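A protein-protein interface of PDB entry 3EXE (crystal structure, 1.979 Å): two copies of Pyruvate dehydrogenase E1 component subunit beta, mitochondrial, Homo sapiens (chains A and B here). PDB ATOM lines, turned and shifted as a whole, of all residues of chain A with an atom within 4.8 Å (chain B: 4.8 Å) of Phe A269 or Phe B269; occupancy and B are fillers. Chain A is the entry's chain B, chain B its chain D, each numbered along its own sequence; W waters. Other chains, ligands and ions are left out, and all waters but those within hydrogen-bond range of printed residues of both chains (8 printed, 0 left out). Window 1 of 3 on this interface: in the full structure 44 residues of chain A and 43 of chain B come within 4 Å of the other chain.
Among the printed residues, merely in contact across the chains: Phe A269 with Gly B137, Gly A137 with Phe B269, Glu A274 with Gln B268, Phe A269 with Met B244, Phe A269 with Gly B270, Gly A270 with Phe B269, Gln A268 with Glu B274, Glu A274 with Ala B273, Ala A273 with Glu B274, Phe A269 with His B138, Met A244 with Phe B269, Pro A267 with Glu B274, Glu A274 with Pro B267, Val A271 with Phe B269, Ala A273 with Ala B273, His A138 with Phe B269, Ile A241 with Phe B269, Phe A269 with Val B271, Phe A269 with Ile B241, Ala A134 with Phe B269, Phe A269 with Ala B134 and Phe A269 with Phe B269.
Met A244 touches Phe B269, and with the chains exchanged Phe A269 touches Met B244.
Pro A267 touches Glu B274, and with the chains exchanged Glu A274 touches Pro B267.
Ala A273 touches its own counterpart, Ala B273.
Ala A273 touches Glu B274, and with the chains exchanged Glu A274 touches Ala B273.
Of the 26 pairs that touch across the chains among the printed residues, 26 have their exchanged pair printed and touching as well.
Printed residues of chain B that touch a printed residue of chain A: Ala B134, Gly B137, His B138, Ile B241, Met B244, Pro B267, Gln B268, Phe B269, Gly B270, Val B271, Ala B273 and Glu B274.
Hydrophobic or aromatic side chains of chain B within 4 Å of the printed part of chain A: His B138, Ile B241, Met B244, Phe B269 and Ala B273.
Among the printed residues, 26 pairs touch across the chains.
Among the printed residues, no Asp or Glu carboxylate lies within 4 Å of a Lys or Arg side-chain nitrogen of the other chain.
Of the printed residues of chain A, Glu B274 touches Pro A267, Gln A268, Phe A269 and Ala A273.
Of the printed residues of chain B, Ala A134 touches Phe B269 (3.8 Å).
Printed residues of chain A within 4 Å of Pro B267: Glu A274 (3.5 Å).
Of the printed residues of chain B, Glu A274 touches Pro B267, Gln B268, Phe B269 and Ala B273.
Printed residues of chain B within 4 Å of Met A244: Phe B269 (3.5 Å).
The nearest printed residue of chain A that does not touch Phe B269 is Ala A273 (5.8 Å).
The nearest printed residue of chain B that does not touch Ala A134 is His B138 (4.4 Å).
Water W6 lies within hydrogen-bond range of the backbone carbonyl oxygen (O) of Phe B269 (2.7 Å) and the backbone carbonyl oxygen (O) of Ala A134 (3.4 Å).
Water W5 bridges O of His B138 and N of Gln A268.
Water W1 lies within hydrogen-bond range of the backbone carbonyl oxygen of His A138 and the backbone NH of Gln B268.
Water W4 lies within hydrogen-bond range of O of Phe A269 (3.0 Å) and O of Ala B134 (3.4 Å).
Water W2 bridges NE2 of His A138 (3.0 Å) and N of Ala B134 (3.3 Å).
Water W3 bridges a ring nitrogen (NE2) of His B138 and the backbone NH (N) of Ala A134.
The backbone carbonyl oxygen (O) of Gln B268 lies within hydrogen-bond range of a ring nitrogen (ND1) of His A138.
The backbone carbonyl oxygen (O) of Gln A268 sits at hydrogen-bond distance from a ring nitrogen (ND1) of His B138 (2.7 Å).
The backbone NH of Phe A269 lies within hydrogen-bond range of the side-chain carboxylate of Glu B274, 2.9 Å away.
The side-chain carboxylate (OE1) of Glu A274 lies within hydrogen-bond range of the backbone NH (N) of Phe B269 (2.8 Å).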
ATOM      1  N   ALA A 134     -10.646 -21.950 -20.791  1.00  0.00           N
ATOM      2  CA  ALA A 134      -9.784 -22.928 -21.481  1.00  0.00           C
ATOM      3  C   ALA A 134     -10.100 -23.073 -22.990  1.00  0.00           C
ATOM      4  O   ALA A 134      -9.165 -23.135 -23.796  1.00  0.00           O
ATOM      5  CB  ALA A 134      -9.800 -24.240 -20.801  1.00  0.00           C
ATOM      6  N   GLY A 137      -8.846 -19.742 -24.502  1.00  0.00           N
ATOM      7  CA  GLY A 137      -7.408 -19.748 -24.267  1.00  0.00           C
ATOM      8  C   GLY A 137      -6.547 -20.589 -25.214  1.00  0.00           C
ATOM      9  O   GLY A 137      -5.332 -20.368 -25.351  1.00  0.00           O
ATOM     10  N   HIS A 138      -7.158 -21.635 -25.765  1.00  0.00           N
ATOM     11  CA  HIS A 138      -6.494 -22.603 -26.574  1.00  0.00           C
ATOM     12  C   HIS A 138      -6.132 -22.058 -27.974  1.00  0.00           C
ATOM     13  O   HIS A 138      -5.290 -22.642 -28.672  1.00  0.00           O
ATOM     14  CB  HIS A 138      -7.566 -23.703 -26.777  1.00  0.00           C
ATOM     15  CG  HIS A 138      -7.138 -24.898 -27.564  1.00  0.00           C
ATOM     16  ND1 HIS A 138      -6.150 -25.772 -27.141  1.00  0.00           N
ATOM     17  CD2 HIS A 138      -7.710 -25.470 -28.650  1.00  0.00           C
ATOM     18  CE1 HIS A 138      -6.104 -26.797 -27.965  1.00  0.00           C
ATOM     19  NE2 HIS A 138      -7.029 -26.636 -28.896  1.00  0.00           N
ATOM     20  N   ILE A 241      -5.709 -15.025 -19.424  1.00  0.00           N
ATOM     21  CA  ILE A 241      -5.680 -16.454 -19.776  1.00  0.00           C
ATOM     22  C   ILE A 241      -4.765 -16.722 -20.987  1.00  0.00           C
ATOM     23  O   ILE A 241      -4.035 -17.722 -21.023  1.00  0.00           O
ATOM     24  CB  ILE A 241      -7.099 -17.000 -20.076  1.00  0.00           C
ATOM     25  CG1 ILE A 241      -8.057 -16.684 -18.906  1.00  0.00           C
ATOM     26  CG2 ILE A 241      -7.062 -18.531 -20.441  1.00  0.00           C
ATOM     27  CD1 ILE A 241      -7.519 -17.309 -17.543  1.00  0.00           C
ATOM     28  N   MET A 244      -0.942 -16.322 -21.079  1.00  0.00           N
ATOM     29  CA  MET A 244      -0.742 -16.305 -19.628  1.00  0.00           C
ATOM     30  C   MET A 244       0.675 -15.942 -19.152  1.00  0.00           C
ATOM     31  O   MET A 244       1.686 -16.241 -19.818  1.00  0.00           O
ATOM     32  CB  MET A 244      -1.183 -17.628 -18.990  1.00  0.00           C
ATOM     33  CG  MET A 244      -0.256 -18.799 -19.228  1.00  0.00           C
ATOM     34  SD  MET A 244      -0.712 -20.119 -18.052  1.00  0.00           S
ATOM     35  CE  MET A 244      -2.095 -20.846 -18.930  1.00  0.00           C
ATOM     36  N   PRO A 267     -12.677 -29.448 -14.874  1.00  0.00           N
ATOM     37  CA  PRO A 267     -11.264 -29.737 -14.652  1.00  0.00           C
ATOM     38  C   PRO A 267     -10.489 -30.236 -15.905  1.00  0.00           C
ATOM     39  O   PRO A 267      -9.310 -29.843 -16.096  1.00  0.00           O
ATOM     40  CB  PRO A 267     -11.303 -30.850 -13.571  1.00  0.00           C
ATOM     41  CG  PRO A 267     -12.626 -31.559 -13.789  1.00  0.00           C
ATOM     42  CD  PRO A 267     -13.586 -30.431 -14.220  1.00  0.00           C
ATOM     43  N   GLN A 268     -11.107 -31.102 -16.729  1.00  0.00           N
ATOM     44  CA  GLN A 268     -10.350 -31.786 -17.769  1.00  0.00           C
ATOM     45  C   GLN A 268     -10.019 -30.852 -18.944  1.00  0.00           C
ATOM     46  O   GLN A 268     -10.920 -30.210 -19.469  1.00  0.00           O
ATOM     47  CB  GLN A 268     -11.062 -33.046 -18.255  1.00  0.00           C
ATOM     48  CG  GLN A 268     -11.297 -34.069 -17.115  1.00  0.00           C
ATOM     49  CD  GLN A 268     -11.690 -35.395 -17.662  1.00  0.00           C
ATOM     50  OE1 GLN A 268     -10.955 -35.967 -18.475  1.00  0.00           O
ATOM     51  NE2 GLN A 268     -12.843 -35.914 -17.234  1.00  0.00           N
ATOM     52  N   PHE A 269      -8.737 -30.759 -19.312  1.00  0.00           N
ATOM     53  CA  PHE A 269      -8.263 -29.832 -20.381  1.00  0.00           C
ATOM     54  C   PHE A 269      -8.585 -28.402 -19.948  1.00  0.00           C
ATOM     55  O   PHE A 269      -8.894 -27.536 -20.780  1.00  0.00           O
ATOM     56  CB  PHE A 269      -8.877 -30.221 -21.769  1.00  0.00           C
ATOM     57  CG  PHE A 269      -8.873 -31.701 -22.009  1.00  0.00           C
ATOM     58  CD1 PHE A 269      -7.728 -32.338 -22.488  1.00  0.00           C
ATOM     59  CD2 PHE A 269     -10.011 -32.475 -21.743  1.00  0.00           C
ATOM     60  CE1 PHE A 269      -7.729 -33.738 -22.653  1.00  0.00           C
ATOM     61  CE2 PHE A 269     -10.022 -33.869 -21.919  1.00  0.00           C
ATOM     62  CZ  PHE A 269      -8.888 -34.512 -22.370  1.00  0.00           C
ATOM     63  N   GLY A 270      -8.524 -28.175 -18.629  1.00  0.00           N
ATOM     64  CA  GLY A 270      -8.901 -26.883 -18.061  1.00  0.00           C
ATOM     65  C   GLY A 270      -7.716 -25.883 -17.950  1.00  0.00           C
ATOM     66  O   GLY A 270      -6.598 -26.130 -18.426  1.00  0.00           O
ATOM     67  N   VAL A 271      -7.940 -24.742 -17.304  1.00  0.00           N
ATOM     68  CA  VAL A 271      -6.878 -23.735 -17.175  1.00  0.00           C
ATOM     69  C   VAL A 271      -5.749 -24.257 -16.248  1.00  0.00           C
ATOM     70  O   VAL A 271      -4.562 -24.069 -16.543  1.00  0.00           O
ATOM     71  CB  VAL A 271      -7.444 -22.380 -16.576  1.00  0.00           C
ATOM     72  CG1 VAL A 271      -6.303 -21.448 -16.207  1.00  0.00           C
ATOM     73  CG2 VAL A 271      -8.454 -21.760 -17.614  1.00  0.00           C
ATOM     74  N   ALA A 273      -4.944 -27.349 -15.829  1.00  0.00           N
ATOM     75  CA  ALA A 273      -4.229 -28.361 -16.625  1.00  0.00           C
ATOM     76  C   ALA A 273      -3.008 -27.709 -17.339  1.00  0.00           C
ATOM     77  O   ALA A 273      -1.866 -28.211 -17.263  1.00  0.00           O
ATOM     78  CB  ALA A 273      -5.204 -29.088 -17.612  1.00  0.00           C
ATOM     79  N   GLU A 274      -3.225 -26.580 -18.001  1.00  0.00           N
ATOM     80  CA  GLU A 274      -2.102 -25.913 -18.723  1.00  0.00           C
ATOM     81  C   GLU A 274      -1.019 -25.379 -17.752  1.00  0.00           C
ATOM     82  O   GLU A 274       0.221 -25.425 -18.033  1.00  0.00           O
ATOM     83  CB  GLU A 274      -2.657 -24.755 -19.599  1.00  0.00           C
ATOM     84  CG  GLU A 274      -1.656 -24.020 -20.505  1.00  0.00           C
ATOM     85  CD  GLU A 274      -0.850 -24.972 -21.388  1.00  0.00           C
ATOM     86  OE1 GLU A 274      -1.379 -26.020 -21.711  1.00  0.00           O
ATOM     87  OE2 GLU A 274       0.286 -24.636 -21.803  1.00  0.00           O
ATOM     88  N   ALA B 134      -9.299 -31.554 -27.441  1.00  0.00           N
ATOM     89  CA  ALA B 134      -9.369 -30.952 -26.112  1.00  0.00           C
ATOM     90  C   ALA B 134     -10.692 -30.158 -25.870  1.00  0.00           C
ATOM     91  O   ALA B 134     -11.238 -30.235 -24.788  1.00  0.00           O
ATOM     92  CB  ALA B 134      -8.106 -30.035 -25.833  1.00  0.00           C
ATOM     93  N   GLY B 137     -13.337 -33.012 -25.404  1.00  0.00           N
ATOM     94  CA  GLY B 137     -12.879 -33.686 -24.179  1.00  0.00           C
ATOM     95  C   GLY B 137     -13.158 -33.030 -22.823  1.00  0.00           C
ATOM     96  O   GLY B 137     -13.203 -33.722 -21.774  1.00  0.00           O
ATOM     97  N   HIS B 138     -13.249 -31.704 -22.853  1.00  0.00           N
ATOM     98  CA  HIS B 138     -13.478 -30.823 -21.697  1.00  0.00           C
ATOM     99  C   HIS B 138     -14.898 -31.030 -21.121  1.00  0.00           C
ATOM    100  O   HIS B 138     -15.140 -30.713 -19.948  1.00  0.00           O
ATOM    101  CB  HIS B 138     -13.309 -29.374 -22.240  1.00  0.00           C
ATOM    102  CG  HIS B 138     -13.404 -28.292 -21.220  1.00  0.00           C
ATOM    103  ND1 HIS B 138     -12.535 -28.180 -20.147  1.00  0.00           N
ATOM    104  CD2 HIS B 138     -14.292 -27.273 -21.105  1.00  0.00           C
ATOM    105  CE1 HIS B 138     -12.858 -27.107 -19.439  1.00  0.00           C
ATOM    106  NE2 HIS B 138     -13.928 -26.539 -19.998  1.00  0.00           N
ATOM    107  N   ILE B 241     -10.515 -40.015 -25.823  1.00  0.00           N
ATOM    108  CA  ILE B 241     -10.104 -38.772 -25.234  1.00  0.00           C
ATOM    109  C   ILE B 241     -10.868 -38.455 -23.904  1.00  0.00           C
ATOM    110  O   ILE B 241     -10.279 -37.937 -22.955  1.00  0.00           O
ATOM    111  CB  ILE B 241     -10.353 -37.633 -26.234  1.00  0.00           C
ATOM    112  CG1 ILE B 241      -9.576 -37.927 -27.537  1.00  0.00           C
ATOM    113  CG2 ILE B 241     -10.074 -36.218 -25.617  1.00  0.00           C
ATOM    114  CD1 ILE B 241      -8.028 -38.004 -27.381  1.00  0.00           C
ATOM    115  N   MET B 244     -10.588 -40.564 -20.630  1.00  0.00           N
ATOM    116  CA  MET B 244      -9.285 -41.155 -21.016  1.00  0.00           C
ATOM    117  C   MET B 244      -8.887 -42.207 -20.005  1.00  0.00           C
ATOM    118  O   MET B 244      -9.282 -42.174 -18.809  1.00  0.00           O
ATOM    119  CB  MET B 244      -8.154 -40.106 -21.170  1.00  0.00           C
ATOM    120  CG  MET B 244      -7.665 -39.505 -19.857  1.00  0.00           C
ATOM    121  SD  MET B 244      -6.274 -38.362 -20.104  1.00  0.00           S
ATOM    122  CE  MET B 244      -7.073 -37.047 -21.079  1.00  0.00           C
ATOM    123  N   PRO B 267      -1.036 -26.423 -28.473  1.00  0.00           N
ATOM    124  CA  PRO B 267      -0.558 -26.926 -27.188  1.00  0.00           C
ATOM    125  C   PRO B 267      -1.349 -26.506 -25.918  1.00  0.00           C
ATOM    126  O   PRO B 267      -1.527 -27.323 -24.992  1.00  0.00           O
ATOM    127  CB  PRO B 267       0.891 -26.367 -27.097  1.00  0.00           C
ATOM    128  CG  PRO B 267       0.954 -25.126 -28.097  1.00  0.00           C
ATOM    129  CD  PRO B 267      -0.074 -25.506 -29.162  1.00  0.00           C
ATOM    130  N   GLN B 268      -1.756 -25.245 -25.864  1.00  0.00           N
ATOM    131  CA  GLN B 268      -2.197 -24.653 -24.599  1.00  0.00           C
ATOM    132  C   GLN B 268      -3.593 -25.151 -24.315  1.00  0.00           C
ATOM    133  O   GLN B 268      -4.448 -25.035 -25.196  1.00  0.00           O
ATOM    134  CB  GLN B 268      -2.178 -23.118 -24.687  1.00  0.00           C
ATOM    135  CG  GLN B 268      -0.763 -22.582 -25.027  1.00  0.00           C
ATOM    136  CD  GLN B 268      -0.670 -21.085 -24.783  1.00  0.00           C
ATOM    137  OE1 GLN B 268      -1.034 -20.617 -23.696  1.00  0.00           O
ATOM    138  NE2 GLN B 268      -0.148 -20.327 -25.754  1.00  0.00           N
ATOM    139  N   PHE B 269      -3.805 -25.748 -23.131  1.00  0.00           N
ATOM    140  CA  PHE B 269      -5.094 -26.299 -22.701  1.00  0.00           C
ATOM    141  C   PHE B 269      -5.431 -27.468 -23.651  1.00  0.00           C
ATOM    142  O   PHE B 269      -6.619 -27.723 -23.963  1.00  0.00           O
ATOM    143  CB  PHE B 269      -6.205 -25.229 -22.683  1.00  0.00           C
ATOM    144  CG  PHE B 269      -5.776 -23.898 -22.062  1.00  0.00           C
ATOM    145  CD1 PHE B 269      -5.740 -23.717 -20.694  1.00  0.00           C
ATOM    146  CD2 PHE B 269      -5.354 -22.853 -22.878  1.00  0.00           C
ATOM    147  CE1 PHE B 269      -5.311 -22.470 -20.146  1.00  0.00           C
ATOM    148  CE2 PHE B 269      -4.906 -21.620 -22.338  1.00  0.00           C
ATOM    149  CZ  PHE B 269      -4.883 -21.446 -20.976  1.00  0.00           C
ATOM    150  N   GLY B 270      -4.362 -28.110 -24.174  1.00  0.00           N
ATOM    151  CA  GLY B 270      -4.532 -29.263 -25.061  1.00  0.00           C
ATOM    152  C   GLY B 270      -4.668 -30.634 -24.423  1.00  0.00           C
ATOM    153  O   GLY B 270      -4.799 -30.778 -23.216  1.00  0.00           O
ATOM    154  N   VAL B 271      -4.589 -31.685 -25.240  1.00  0.00           N
ATOM    155  CA  VAL B 271      -4.697 -33.021 -24.677  1.00  0.00           C
ATOM    156  C   VAL B 271      -3.494 -33.343 -23.749  1.00  0.00           C
ATOM    157  O   VAL B 271      -3.682 -33.901 -22.650  1.00  0.00           O
ATOM    158  CB  VAL B 271      -4.823 -34.093 -25.800  1.00  0.00           C
ATOM    159  CG1 VAL B 271      -4.860 -35.487 -25.200  1.00  0.00           C
ATOM    160  CG2 VAL B 271      -6.106 -33.770 -26.600  1.00  0.00           C
ATOM    161  N   ALA B 273      -1.575 -31.341 -22.054  1.00  0.00           N
ATOM    162  CA  ALA B 273      -1.735 -30.619 -20.768  1.00  0.00           C
ATOM    163  C   ALA B 273      -2.508 -31.438 -19.719  1.00  0.00           C
ATOM    164  O   ALA B 273      -2.100 -31.558 -18.548  1.00  0.00           O
ATOM    165  CB  ALA B 273      -2.438 -29.229 -20.969  1.00  0.00           C
ATOM    166  N   GLU B 274      -3.637 -31.987 -20.115  1.00  0.00           N
ATOM    167  CA  GLU B 274      -4.451 -32.783 -19.180  1.00  0.00           C
ATOM    168  C   GLU B 274      -3.699 -34.048 -18.723  1.00  0.00           C
ATOM    169  O   GLU B 274      -3.703 -34.375 -17.539  1.00  0.00           O
ATOM    170  CB  GLU B 274      -5.859 -33.130 -19.783  1.00  0.00           C
ATOM    171  CG  GLU B 274      -6.767 -33.994 -18.847  1.00  0.00           C
ATOM    172  CD  GLU B 274      -7.048 -33.335 -17.509  1.00  0.00           C
ATOM    173  OE1 GLU B 274      -6.944 -32.089 -17.448  1.00  0.00           O
ATOM    174  OE2 GLU B 274      -7.408 -34.045 -16.531  1.00  0.00           O
HETATM  175  O   HOH W   1      -2.507 -23.026 -27.891  1.00  0.00           O
HETATM  176  O   HOH W   2      -9.294 -28.661 -29.033  1.00  0.00           O
HETATM  177  O   HOH W   3     -13.381 -23.788 -21.402  1.00  0.00           O
HETATM  178  O   HOH W   4     -10.741 -27.333 -23.181  1.00  0.00           O
HETATM  179  O   HOH W   5     -13.882 -31.847 -17.577  1.00  0.00           O
HETATM  180  O   HOH W   6      -8.852 -26.387 -24.824  1.00  0.00           O
HETATM  181  O   HOH W   7     -10.927 -37.769 -20.181  1.00  0.00           O
HETATM  182  O   HOH W   8      -1.803 -18.675 -22.267  1.00  0.00           O
